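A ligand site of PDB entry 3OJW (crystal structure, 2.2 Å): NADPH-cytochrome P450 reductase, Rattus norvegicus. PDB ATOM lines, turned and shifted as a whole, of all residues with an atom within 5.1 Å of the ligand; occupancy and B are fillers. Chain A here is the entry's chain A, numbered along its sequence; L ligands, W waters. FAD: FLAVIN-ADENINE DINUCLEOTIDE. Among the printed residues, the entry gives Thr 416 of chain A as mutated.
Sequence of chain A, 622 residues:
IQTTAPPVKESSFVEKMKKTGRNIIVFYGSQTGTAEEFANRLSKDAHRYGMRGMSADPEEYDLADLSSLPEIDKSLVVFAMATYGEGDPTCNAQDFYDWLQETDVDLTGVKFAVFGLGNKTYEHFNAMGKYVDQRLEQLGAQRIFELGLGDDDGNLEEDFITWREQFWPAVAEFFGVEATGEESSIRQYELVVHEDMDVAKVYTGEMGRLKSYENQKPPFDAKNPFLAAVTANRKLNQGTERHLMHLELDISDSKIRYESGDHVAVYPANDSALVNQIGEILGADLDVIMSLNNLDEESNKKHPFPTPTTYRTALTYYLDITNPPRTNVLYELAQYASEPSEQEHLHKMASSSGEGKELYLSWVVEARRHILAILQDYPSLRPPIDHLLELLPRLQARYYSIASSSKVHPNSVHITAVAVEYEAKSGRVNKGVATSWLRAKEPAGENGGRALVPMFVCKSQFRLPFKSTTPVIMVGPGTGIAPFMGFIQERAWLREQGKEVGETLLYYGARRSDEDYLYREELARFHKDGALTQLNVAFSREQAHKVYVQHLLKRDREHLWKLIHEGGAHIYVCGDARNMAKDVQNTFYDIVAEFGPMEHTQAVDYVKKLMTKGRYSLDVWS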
ATOM      1  N   GLN A  31       8.634  11.691 -22.461  1.00  0.00           N
ATOM      2  CA  GLN A  31       9.376  12.892 -22.823  1.00  0.00           C
ATOM      3  C   GLN A  31       8.986  14.046 -21.891  1.00  0.00           C
ATOM      4  O   GLN A  31       9.813  14.900 -21.609  1.00  0.00           O
ATOM      5  CB  GLN A  31       9.137  13.264 -24.281  1.00  0.00           C
ATOM      6  CG  GLN A  31      10.176  14.223 -24.822  1.00  0.00           C
ATOM      7  CD  GLN A  31      10.488  13.966 -26.286  1.00  0.00           C
ATOM      8  OE1 GLN A  31      10.982  12.896 -26.657  1.00  0.00           O
ATOM      9  NE2 GLN A  31      10.195  14.952 -27.131  1.00  0.00           N
ATOM     10  N   HIS A 263      17.428  17.686 -32.231  1.00  0.00           N
ATOM     11  CA  HIS A 263      16.932  18.534 -31.160  1.00  0.00           C
ATOM     12  C   HIS A 263      17.941  18.593 -30.033  1.00  0.00           C
ATOM     13  O   HIS A 263      18.687  17.651 -29.809  1.00  0.00           O
ATOM     14  CB  HIS A 263      15.616  17.989 -30.614  1.00  0.00           C
ATOM     15  CG  HIS A 263      14.515  17.941 -31.623  1.00  0.00           C
ATOM     16  ND1 HIS A 263      13.872  16.763 -31.963  1.00  0.00           N
ATOM     17  CD2 HIS A 263      13.935  18.914 -32.362  1.00  0.00           C
ATOM     18  CE1 HIS A 263      12.943  17.027 -32.866  1.00  0.00           C
ATOM     19  NE2 HIS A 263      12.960  18.319 -33.129  1.00  0.00           N
ATOM     20  N   THR A 322       5.306  25.288 -12.144  1.00  0.00           N
ATOM     21  CA  THR A 322       4.648  26.235 -13.033  1.00  0.00           C
ATOM     22  C   THR A 322       3.410  25.729 -13.766  1.00  0.00           C
ATOM     23  O   THR A 322       2.554  26.521 -14.158  1.00  0.00           O
ATOM     24  CB  THR A 322       5.648  26.797 -14.060  1.00  0.00           C
ATOM     25  OG1 THR A 322       6.343  25.716 -14.698  1.00  0.00           O
ATOM     26  CG2 THR A 322       6.655  27.700 -13.362  1.00  0.00           C
ATOM     27  N   ASN A 323       3.282  24.418 -13.957  1.00  0.00           N
ATOM     28  CA  ASN A 323       2.122  23.875 -14.661  1.00  0.00           C
ATOM     29  C   ASN A 323       0.917  23.661 -13.744  1.00  0.00           C
ATOM     30  O   ASN A 323       1.048  23.669 -12.525  1.00  0.00           O
ATOM     31  CB  ASN A 323       2.484  22.572 -15.376  1.00  0.00           C
ATOM     32  CG  ASN A 323       3.391  22.816 -16.551  1.00  0.00           C
ATOM     33  OD1 ASN A 323       3.139  23.696 -17.371  1.00  0.00           O
ATOM     34  ND2 ASN A 323       4.472  22.042 -16.654  1.00  0.00           N
ATOM     35  N   ARG A 368      -4.506  28.510 -16.184  1.00  0.00           N
ATOM     36  CA  ARG A 368      -3.084  28.276 -15.971  1.00  0.00           C
ATOM     37  C   ARG A 368      -2.570  28.632 -14.568  1.00  0.00           C
ATOM     38  O   ARG A 368      -1.534  29.279 -14.432  1.00  0.00           O
ATOM     39  CB  ARG A 368      -2.256  29.014 -17.023  1.00  0.00           C
ATOM     40  CG  ARG A 368      -2.437  28.533 -18.482  1.00  0.00           C
ATOM     41  CD  ARG A 368      -1.819  27.148 -18.739  1.00  0.00           C
ATOM     42  NE  ARG A 368      -0.385  27.097 -18.460  1.00  0.00           N
ATOM     43  CZ  ARG A 368       0.357  25.986 -18.462  1.00  0.00           C
ATOM     44  NH1 ARG A 368       1.646  26.037 -18.186  1.00  0.00           N
ATOM     45  NH2 ARG A 368      -0.207  24.812 -18.749  1.00  0.00           N
ATOM     46  N   ARG A 398      13.448  20.885 -21.735  1.00  0.00           N
ATOM     47  CA  ARG A 398      12.749  21.542 -22.839  1.00  0.00           C
ATOM     48  C   ARG A 398      13.553  21.282 -24.109  1.00  0.00           C
ATOM     49  O   ARG A 398      14.793  21.393 -24.104  1.00  0.00           O
ATOM     50  CB  ARG A 398      12.640  23.059 -22.603  1.00  0.00           C
ATOM     51  CG  ARG A 398      11.365  23.514 -21.908  1.00  0.00           C
ATOM     52  CD  ARG A 398      11.247  22.973 -20.486  1.00  0.00           C
ATOM     53  NE  ARG A 398      10.071  23.540 -19.816  1.00  0.00           N
ATOM     54  CZ  ARG A 398       9.664  23.220 -18.591  1.00  0.00           C
ATOM     55  NH1 ARG A 398       8.578  23.799 -18.099  1.00  0.00           N
ATOM     56  NH2 ARG A 398      10.323  22.329 -17.853  1.00  0.00           N
ATOM     57  N   TYR A 399      12.851  20.943 -25.185  1.00  0.00           N
ATOM     58  CA  TYR A 399      13.477  20.644 -26.463  1.00  0.00           C
ATOM     59  C   TYR A 399      13.433  21.781 -27.468  1.00  0.00           C
ATOM     60  O   TYR A 399      12.444  22.518 -27.562  1.00  0.00           O
ATOM     61  CB  TYR A 399      12.827  19.395 -27.069  1.00  0.00           C
ATOM     62  CG  TYR A 399      13.140  18.144 -26.280  1.00  0.00           C
ATOM     63  CD1 TYR A 399      14.083  17.232 -26.732  1.00  0.00           C
ATOM     64  CD2 TYR A 399      12.508  17.893 -25.057  1.00  0.00           C
ATOM     65  CE1 TYR A 399      14.420  16.108 -25.995  1.00  0.00           C
ATOM     66  CE2 TYR A 399      12.835  16.767 -24.298  1.00  0.00           C
ATOM     67  CZ  TYR A 399      13.794  15.879 -24.781  1.00  0.00           C
ATOM     68  OH  TYR A 399      14.152  14.776 -24.046  1.00  0.00           O
ATOM     69  N   TYR A 400      14.524  21.923 -28.228  1.00  0.00           N
ATOM     70  CA  TYR A 400      14.635  22.961 -29.253  1.00  0.00           C
ATOM     71  C   TYR A 400      15.247  22.384 -30.526  1.00  0.00           C
ATOM     72  O   TYR A 400      16.080  21.474 -30.467  1.00  0.00           O
ATOM     73  CB  TYR A 400      15.509  24.101 -28.726  1.00  0.00           C
ATOM     74  CG  TYR A 400      14.862  24.795 -27.563  1.00  0.00           C
ATOM     75  CD1 TYR A 400      13.908  25.780 -27.761  1.00  0.00           C
ATOM     76  CD2 TYR A 400      15.142  24.397 -26.251  1.00  0.00           C
ATOM     77  CE1 TYR A 400      13.232  26.341 -26.711  1.00  0.00           C
ATOM     78  CE2 TYR A 400      14.460  24.950 -25.190  1.00  0.00           C
ATOM     79  CZ  TYR A 400      13.508  25.926 -25.425  1.00  0.00           C
ATOM     80  OH  TYR A 400      12.773  26.411 -24.377  1.00  0.00           O
ATOM     81  N   SER A 401      14.830  22.917 -31.673  1.00  0.00           N
ATOM     82  CA  SER A 401      15.367  22.444 -32.950  1.00  0.00           C
ATOM     83  C   SER A 401      16.705  23.120 -33.202  1.00  0.00           C
ATOM     84  O   SER A 401      16.777  24.339 -33.319  1.00  0.00           O
ATOM     85  CB  SER A 401      14.414  22.792 -34.101  1.00  0.00           C
ATOM     86  OG  SER A 401      13.166  22.151 -33.931  1.00  0.00           O
ATOM     87  N   THR A 416      16.884  28.811 -31.651  1.00  0.00           N
ATOM     88  CA  THR A 416      16.042  29.919 -32.065  1.00  0.00           C
ATOM     89  C   THR A 416      14.777  29.768 -31.226  1.00  0.00           C
ATOM     90  O   THR A 416      14.087  28.745 -31.310  1.00  0.00           O
ATOM     91  CB  THR A 416      15.640  29.812 -33.562  1.00  0.00           C
ATOM     92  OG1 THR A 416      16.815  29.851 -34.382  1.00  0.00           O
ATOM     93  CG2 THR A 416      14.729  30.957 -33.953  1.00  0.00           C
ATOM     94  N   ALA A 417      14.444  30.779 -30.419  1.00  0.00           N
ATOM     95  CA  ALA A 417      13.262  30.652 -29.576  1.00  0.00           C
ATOM     96  C   ALA A 417      12.610  31.944 -29.146  1.00  0.00           C
ATOM     97  O   ALA A 417      13.265  32.963 -28.966  1.00  0.00           O
ATOM     98  CB  ALA A 417      13.607  29.840 -28.348  1.00  0.00           C
ATOM     99  N   VAL A 418      11.301  31.892 -28.974  1.00  0.00           N
ATOM    100  CA  VAL A 418      10.543  33.036 -28.514  1.00  0.00           C
ATOM    101  C   VAL A 418      10.363  32.901 -27.003  1.00  0.00           C
ATOM    102  O   VAL A 418      10.026  31.838 -26.506  1.00  0.00           O
ATOM    103  CB  VAL A 418       9.162  33.110 -29.206  1.00  0.00           C
ATOM    104  CG1 VAL A 418       8.386  31.834 -28.961  1.00  0.00           C
ATOM    105  CG2 VAL A 418       8.386  34.301 -28.659  1.00  0.00           C
ATOM    106  N   VAL A 420       8.628  32.939 -23.594  1.00  0.00           N
ATOM    107  CA  VAL A 420       7.223  32.765 -23.217  1.00  0.00           C
ATOM    108  C   VAL A 420       6.833  33.604 -22.010  1.00  0.00           C
ATOM    109  O   VAL A 420       7.428  33.485 -20.937  1.00  0.00           O
ATOM    110  CB  VAL A 420       6.910  31.279 -22.930  1.00  0.00           C
ATOM    111  CG1 VAL A 420       5.488  31.127 -22.388  1.00  0.00           C
ATOM    112  CG2 VAL A 420       7.075  30.485 -24.218  1.00  0.00           C
ATOM    113  N   TYR A 422       2.967  35.601 -20.580  1.00  0.00           N
ATOM    114  CA  TYR A 422       1.581  35.968 -20.843  1.00  0.00           C
ATOM    115  C   TYR A 422       0.764  36.208 -19.576  1.00  0.00           C
ATOM    116  O   TYR A 422       1.117  35.772 -18.492  1.00  0.00           O
ATOM    117  CB  TYR A 422       0.891  34.869 -21.643  1.00  0.00           C
ATOM    118  CG  TYR A 422       0.892  33.531 -20.929  1.00  0.00           C
ATOM    119  CD1 TYR A 422       2.004  32.699 -20.985  1.00  0.00           C
ATOM    120  CD2 TYR A 422      -0.199  33.118 -20.181  1.00  0.00           C
ATOM    121  CE1 TYR A 422       2.026  31.472 -20.308  1.00  0.00           C
ATOM    122  CE2 TYR A 422      -0.193  31.890 -19.494  1.00  0.00           C
ATOM    123  CZ  TYR A 422       0.924  31.081 -19.558  1.00  0.00           C
ATOM    124  OH  TYR A 422       0.949  29.896 -18.875  1.00  0.00           O
ATOM    125  N   LYS A 431       5.469  33.013 -16.664  1.00  0.00           N
ATOM    126  CA  LYS A 431       6.742  33.071 -17.398  1.00  0.00           C
ATOM    127  C   LYS A 431       7.177  31.668 -17.823  1.00  0.00           C
ATOM    128  O   LYS A 431       7.158  30.748 -17.027  1.00  0.00           O
ATOM    129  CB  LYS A 431       7.825  33.673 -16.512  1.00  0.00           C
ATOM    130  CG  LYS A 431       7.502  35.050 -15.942  1.00  0.00           C
ATOM    131  CD  LYS A 431       7.463  36.106 -17.040  1.00  0.00           C
ATOM    132  CE  LYS A 431       8.791  36.197 -17.777  1.00  0.00           C
ATOM    133  NZ  LYS A 431       9.921  36.521 -16.865  1.00  0.00           N
ATOM    134  N   GLY A 432       7.565  31.522 -19.080  1.00  0.00           N
ATOM    135  CA  GLY A 432       8.030  30.216 -19.548  1.00  0.00           C
ATOM    136  C   GLY A 432       9.250  29.881 -18.709  1.00  0.00           C
ATOM    137  O   GLY A 432      10.093  30.747 -18.477  1.00  0.00           O
ATOM    138  N   VAL A 433       9.355  28.642 -18.243  1.00  0.00           N
ATOM    139  CA  VAL A 433      10.500  28.283 -17.412  1.00  0.00           C
ATOM    140  C   VAL A 433      11.853  28.320 -18.132  1.00  0.00           C
ATOM    141  O   VAL A 433      12.762  29.052 -17.720  1.00  0.00           O
ATOM    142  CB  VAL A 433      10.314  26.893 -16.777  1.00  0.00           C
ATOM    143  CG1 VAL A 433      11.567  26.531 -15.962  1.00  0.00           C
ATOM    144  CG2 VAL A 433       9.063  26.878 -15.890  1.00  0.00           C
ATOM    145  N   ALA A 434      12.000  27.547 -19.196  1.00  0.00           N
ATOM    146  CA  ALA A 434      13.256  27.476 -19.925  1.00  0.00           C
ATOM    147  C   ALA A 434      13.612  28.752 -20.691  1.00  0.00           C
ATOM    148  O   ALA A 434      14.755  29.216 -20.617  1.00  0.00           O
ATOM    149  CB  ALA A 434      13.259  26.275 -20.880  1.00  0.00           C
ATOM    150  N   THR A 435      12.658  29.310 -21.429  1.00  0.00           N
ATOM    151  CA  THR A 435      12.956  30.525 -22.196  1.00  0.00           C
ATOM    152  C   THR A 435      13.293  31.718 -21.316  1.00  0.00           C
ATOM    153  O   THR A 435      14.064  32.576 -21.744  1.00  0.00           O
ATOM    154  CB  THR A 435      11.804  30.901 -23.153  1.00  0.00           C
ATOM    155  OG1 THR A 435      10.591  31.038 -22.407  1.00  0.00           O
ATOM    156  CG2 THR A 435      11.624  29.823 -24.211  1.00  0.00           C
ATOM    157  N   SER A 436      12.740  31.793 -20.103  1.00  0.00           N
ATOM    158  CA  SER A 436      13.067  32.906 -19.205  1.00  0.00           C
ATOM    159  C   SER A 436      14.494  32.698 -18.714  1.00  0.00           C
ATOM    160  O   SER A 436      15.273  33.636 -18.564  1.00  0.00           O
ATOM    161  CB  SER A 436      12.123  32.953 -18.002  1.00  0.00           C
ATOM    162  OG  SER A 436      10.824  33.365 -18.370  1.00  0.00           O
ATOM    163  N   THR A 479       9.460  31.044 -35.733  1.00  0.00           N
ATOM    164  CA  THR A 479      10.582  30.271 -35.208  1.00  0.00           C
ATOM    165  C   THR A 479      10.744  28.907 -35.870  1.00  0.00           C
ATOM    166  O   THR A 479      11.782  28.268 -35.731  1.00  0.00           O
ATOM    167  CB  THR A 479      10.453  30.058 -33.675  1.00  0.00           C
ATOM    168  OG1 THR A 479       9.198  29.444 -33.380  1.00  0.00           O
ATOM    169  CG2 THR A 479      10.552  31.392 -32.952  1.00  0.00           C
ATOM    170  N   ALA A 482      14.012  27.642 -37.616  1.00  0.00           N
ATOM    171  CA  ALA A 482      15.184  27.107 -36.923  1.00  0.00           C
ATOM    172  C   ALA A 482      15.941  25.953 -37.578  1.00  0.00           C
ATOM    173  O   ALA A 482      17.099  26.113 -37.957  1.00  0.00           O
ATOM    174  CB  ALA A 482      14.793  26.717 -35.502  1.00  0.00           C
ATOM    175  N   ASP A 619       8.033  18.513 -38.198  1.00  0.00           N
ATOM    176  CA  ASP A 619       8.599  18.809 -36.904  1.00  0.00           C
ATOM    177  C   ASP A 619       7.727  19.905 -36.306  1.00  0.00           C
ATOM    178  O   ASP A 619       8.075  21.079 -36.356  1.00  0.00           O
ATOM    179  CB  ASP A 619      10.050  19.268 -37.019  1.00  0.00           C
ATOM    180  CG  ASP A 619      10.729  19.350 -35.662  1.00  0.00           C
ATOM    181  OD1 ASP A 619      10.675  18.352 -34.909  1.00  0.00           O
ATOM    182  OD2 ASP A 619      11.324  20.404 -35.348  1.00  0.00           O
ATOM    183  N   TRP A 621       6.030  21.356 -33.002  1.00  0.00           N
ATOM    184  CA  TRP A 621       6.332  21.364 -31.578  1.00  0.00           C
ATOM    185  C   TRP A 621       5.203  21.262 -30.570  1.00  0.00           C
ATOM    186  O   TRP A 621       5.450  21.345 -29.368  1.00  0.00           O
ATOM    187  CB  TRP A 621       7.145  22.609 -31.281  1.00  0.00           C
ATOM    188  CG  TRP A 621       8.225  22.880 -32.305  1.00  0.00           C
ATOM    189  CD1 TRP A 621       8.933  21.950 -33.011  1.00  0.00           C
ATOM    190  CD2 TRP A 621       8.762  24.155 -32.655  1.00  0.00           C
ATOM    191  NE1 TRP A 621       9.891  22.572 -33.776  1.00  0.00           N
ATOM    192  CE2 TRP A 621       9.799  23.923 -33.579  1.00  0.00           C
ATOM    193  CE3 TRP A 621       8.455  25.471 -32.274  1.00  0.00           C
ATOM    194  CZ2 TRP A 621      10.548  24.970 -34.130  1.00  0.00           C
ATOM    195  CZ3 TRP A 621       9.203  26.505 -32.826  1.00  0.00           C
ATOM    196  CH2 TRP A 621      10.231  26.244 -33.748  1.00  0.00           C
HETATM  197  PA  FAD L   1       6.833  26.550 -20.064  1.00  0.00           P
HETATM  198  O1A FAD L   1       7.095  27.130 -18.738  1.00  0.00           O
HETATM  199  O2A FAD L   1       7.025  25.131 -20.217  1.00  0.00           O
HETATM  200  O5B FAD L   1       5.356  26.924 -20.556  1.00  0.00           O
HETATM  201  C5B FAD L   1       4.771  26.508 -21.808  1.00  0.00           C
HETATM  202  C4B FAD L   1       3.289  26.232 -21.602  1.00  0.00           C
HETATM  203  O4B FAD L   1       2.637  27.448 -21.235  1.00  0.00           O
HETATM  204  C3B FAD L   1       2.554  25.754 -22.856  1.00  0.00           C
HETATM  205  O3B FAD L   1       2.639  24.341 -23.009  1.00  0.00           O
HETATM  206  C2B FAD L   1       1.131  26.225 -22.653  1.00  0.00           C
HETATM  207  O2B FAD L   1       0.299  25.255 -22.005  1.00  0.00           O
HETATM  208  C1B FAD L   1       1.333  27.482 -21.822  1.00  0.00           C
HETATM  209  N9A FAD L   1       1.216  28.787 -22.554  1.00  0.00           N
HETATM  210  C8A FAD L   1       2.074  29.527 -23.365  1.00  0.00           C
HETATM  211  N7A FAD L   1       1.653  30.713 -23.889  1.00  0.00           N
HETATM  212  C5A FAD L   1       0.352  30.719 -23.353  1.00  0.00           C
HETATM  213  C6A FAD L   1      -0.748  31.635 -23.449  1.00  0.00           C
HETATM  214  N6A FAD L   1      -0.669  32.760 -24.155  1.00  0.00           N
HETATM  215  N1A FAD L   1      -1.952  31.361 -22.784  1.00  0.00           N
HETATM  216  C2A FAD L   1      -2.111  30.203 -22.018  1.00  0.00           C
HETATM  217  N3A FAD L   1      -1.145  29.250 -21.855  1.00  0.00           N
HETATM  218  C4A FAD L   1       0.079  29.554 -22.544  1.00  0.00           C
HETATM  219  N1  FAD L   1      10.389  26.360 -29.122  1.00  0.00           N
HETATM  220  C2  FAD L   1      11.113  27.369 -29.697  1.00  0.00           C
HETATM  221  O2  FAD L   1      10.916  28.520 -29.352  1.00  0.00           O
HETATM  222  N3  FAD L   1      12.061  26.963 -30.679  1.00  0.00           N
HETATM  223  C4  FAD L   1      12.330  25.643 -31.122  1.00  0.00           C
HETATM  224  O4  FAD L   1      13.183  25.476 -31.981  1.00  0.00           O
HETATM  225  C4X FAD L   1      11.509  24.587 -30.478  1.00  0.00           C
HETATM  226  N5  FAD L   1      11.710  23.252 -30.882  1.00  0.00           N
HETATM  227  C5X FAD L   1      10.904  22.246 -30.248  1.00  0.00           C
HETATM  228  C6  FAD L   1      11.103  20.857 -30.677  1.00  0.00           C
HETATM  229  C7  FAD L   1      10.363  19.745 -30.134  1.00  0.00           C
HETATM  230  C7M FAD L   1      10.608  18.311 -30.623  1.00  0.00           C
HETATM  231  C8  FAD L   1       9.304  20.072 -29.048  1.00  0.00           C
HETATM  232  C8M FAD L   1       8.410  18.994 -28.371  1.00  0.00           C
HETATM  233  C9  FAD L   1       9.110  21.392 -28.634  1.00  0.00           C
HETATM  234  C9A FAD L   1       9.868  22.503 -29.187  1.00  0.00           C
HETATM  235  N10 FAD L   1       9.719  23.930 -28.792  1.00  0.00           N
HETATM  236  C10 FAD L   1      10.547  25.011 -29.461  1.00  0.00           C
HETATM  237  C1' FAD L   1       8.779  24.426 -27.733  1.00  0.00           C
HETATM  238  C2' FAD L   1       9.862  24.235 -26.535  1.00  0.00           C
HETATM  239  O2' FAD L   1      10.153  22.843 -26.175  1.00  0.00           O
HETATM  240  C3' FAD L   1       9.375  24.963 -25.204  1.00  0.00           C
HETATM  241  O3' FAD L   1       8.112  24.374 -24.882  1.00  0.00           O
HETATM  242  C4' FAD L   1       9.046  26.473 -25.254  1.00  0.00           C
HETATM  243  O4' FAD L   1      10.285  27.089 -25.556  1.00  0.00           O
HETATM  244  C5' FAD L   1       8.593  27.059 -23.892  1.00  0.00           C
HETATM  245  O5' FAD L   1       9.194  26.472 -22.792  1.00  0.00           O
HETATM  246  P   FAD L   1       9.216  27.201 -21.411  1.00  0.00           P
HETATM  247  O1P FAD L   1       9.905  26.287 -20.470  1.00  0.00           O
HETATM  248  O2P FAD L   1       9.859  28.555 -21.545  1.00  0.00           O
HETATM  249  O3P FAD L   1       7.705  27.303 -21.141  1.00  0.00           O
HETATM  250  O   HOH W   1       3.397  28.581 -18.639  1.00  0.00           O
HETATM  251  O   HOH W   2       7.079  28.853 -26.869  1.00  0.00           O
HETATM  252  O   HOH W   3       5.700  25.243 -16.995  1.00  0.00           O
HETATM  253  O   HOH W   4      10.063  20.607 -24.802  1.00  0.00           O
HETATM  254  O   HOH W   5      -4.674  31.947 -21.576  1.00  0.00           O
HETATM  255  O   HOH W   6       5.415  28.819 -17.171  1.00  0.00           O
HETATM  256  O   HOH W   7       5.839  22.742 -19.288  1.00  0.00           O
HETATM  257  O   HOH W   8      15.731  26.236 -31.854  1.00  0.00           O
HETATM  258  O   HOH W   9       7.612  23.244 -22.322  1.00  0.00           O
HETATM  259  O   HOH W  10       9.647  29.046 -27.217  1.00  0.00           O
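Water W10 bridges O2 of the ligand and O of Val 418.
Water W4 lies within hydrogen-bond range of O2' of the ligand and N of Tyr 399.
Water W8 lies within hydrogen-bond range of the backbone carbonyl oxygen (O) of Ser 401 (2.6 Å), an oxygen (O4) of the ligand (2.7 Å) and the backbone NH (N) of Thr 416 (2.8 Å).
Water W6 lies within hydrogen-bond range of the backbone carbonyl oxygen (O) of Lys 431 (2.6 Å) and an oxygen (O1A) of the ligand (2.9 Å).
Water W3 lies within hydrogen-bond range of the side-chain hydroxyl of Thr 322 (2.4 Å), an oxygen (O1A) of the ligand (2.9 Å), the side-chain amide oxygen of Asn 323 (3.0 Å) and the guanidinium group of Arg 398 (3.4 Å).
Water W1 lies within hydrogen-bond range of the side-chain hydroxyl of Tyr 422, an oxygen (O4B) of the ligand and the guanidinium group of Arg 368.
O2P of the ligand lies within hydrogen-bond range of OG1 of Thr 435, at 2.7 Å.
An oxygen (O2') of the ligand is in hydrogen-bond range of the backbone NH (N) of Tyr 399, 3.4 Å away.
An oxygen (O4') of the ligand sits at hydrogen-bond distance from the side-chain hydroxyl of Tyr 400, at 2.8 Å.
The backbone carbonyl oxygen (O) of Tyr 399 is in hydrogen-bond range of an oxygen (O2') of the ligand (2.7 Å).
NH2 of Arg 368 is in hydrogen-bond range of O2B of the ligand (3.3 Å).
O4 of the ligand is in hydrogen-bond range of N of Ser 401 (3.1 Å).
NE1 of Trp 621 sits close to N5 of the ligand (3.5 Å).
O of Thr 416 lies within hydrogen-bond range of N3 of the ligand (2.8 Å).
NE of Arg 398 is in salt-bridge range of O1P of the ligand.
The backbone NH of Thr 435 sits at hydrogen-bond distance from an oxygen (O2P) of the ligand.
N of Ala 434 sits at hydrogen-bond distance from O1P of the ligand.
An oxygen (O2) of the ligand lies within hydrogen-bond range of the backbone NH (N) of Val 418, at 3.4 Å.
O1A of the ligand is in hydrogen-bond range of N of Val 433 (2.8 Å).
Merely in contact with the ligand: His 263 (3.4 Å), Ala 417 (3.2 Å), Val 420 (3.8 Å), Tyr 422 (3.5 Å) and Gly 432 (3.2 Å).
Hydrophobic or aromatic side chains that line the ligand: His 263, Tyr 399, Tyr 400, Ala 417, Val 420, Tyr 422, Val 433, Ala 434 and Trp 621.
16 residues have an atom within 4 Å of the ligand: His 263, Arg 368, Arg 398, Tyr 399, Tyr 400, Ser 401, Thr 416, Ala 417, Val 418, Val 420, Tyr 422, Gly 432, Val 433, Ala 434, Thr 435 and Trp 621.
The nearest printed residue that does not touch the ligand is Lys 431 (4.003 Å).
OD2 of Asp 619 sits at hydrogen-bond distance from NE1 of Trp 621.
The backbone carbonyl oxygen (O) of Val 420 sits at hydrogen-bond distance from the backbone NH (N) of Gly 432, 2.7 Å away.
OH of Tyr 422 lies within hydrogen-bond range of NE of Arg 368, at 3.1 Å.
The backbone carbonyl oxygen (O) of Gly 432 is in hydrogen-bond range of the side-chain hydroxyl (OG) of Ser 436 (2.7 Å).
The backbone NH (N) of Val 420 lies within hydrogen-bond range of the side-chain hydroxyl (OG1) of Thr 435 (3.0 Å).
The side-chain hydroxyl (OG) of Ser 401 is in hydrogen-bond range of the side-chain carboxylate (OD2) of Asp 619 (2.9 Å).
NH1 of Arg 368 sits at hydrogen-bond distance from OD1 of Asn 323, 2.9 Å away.
OG of Ser 401 lies within hydrogen-bond range of NE1 of Trp 621 (3.3 Å).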
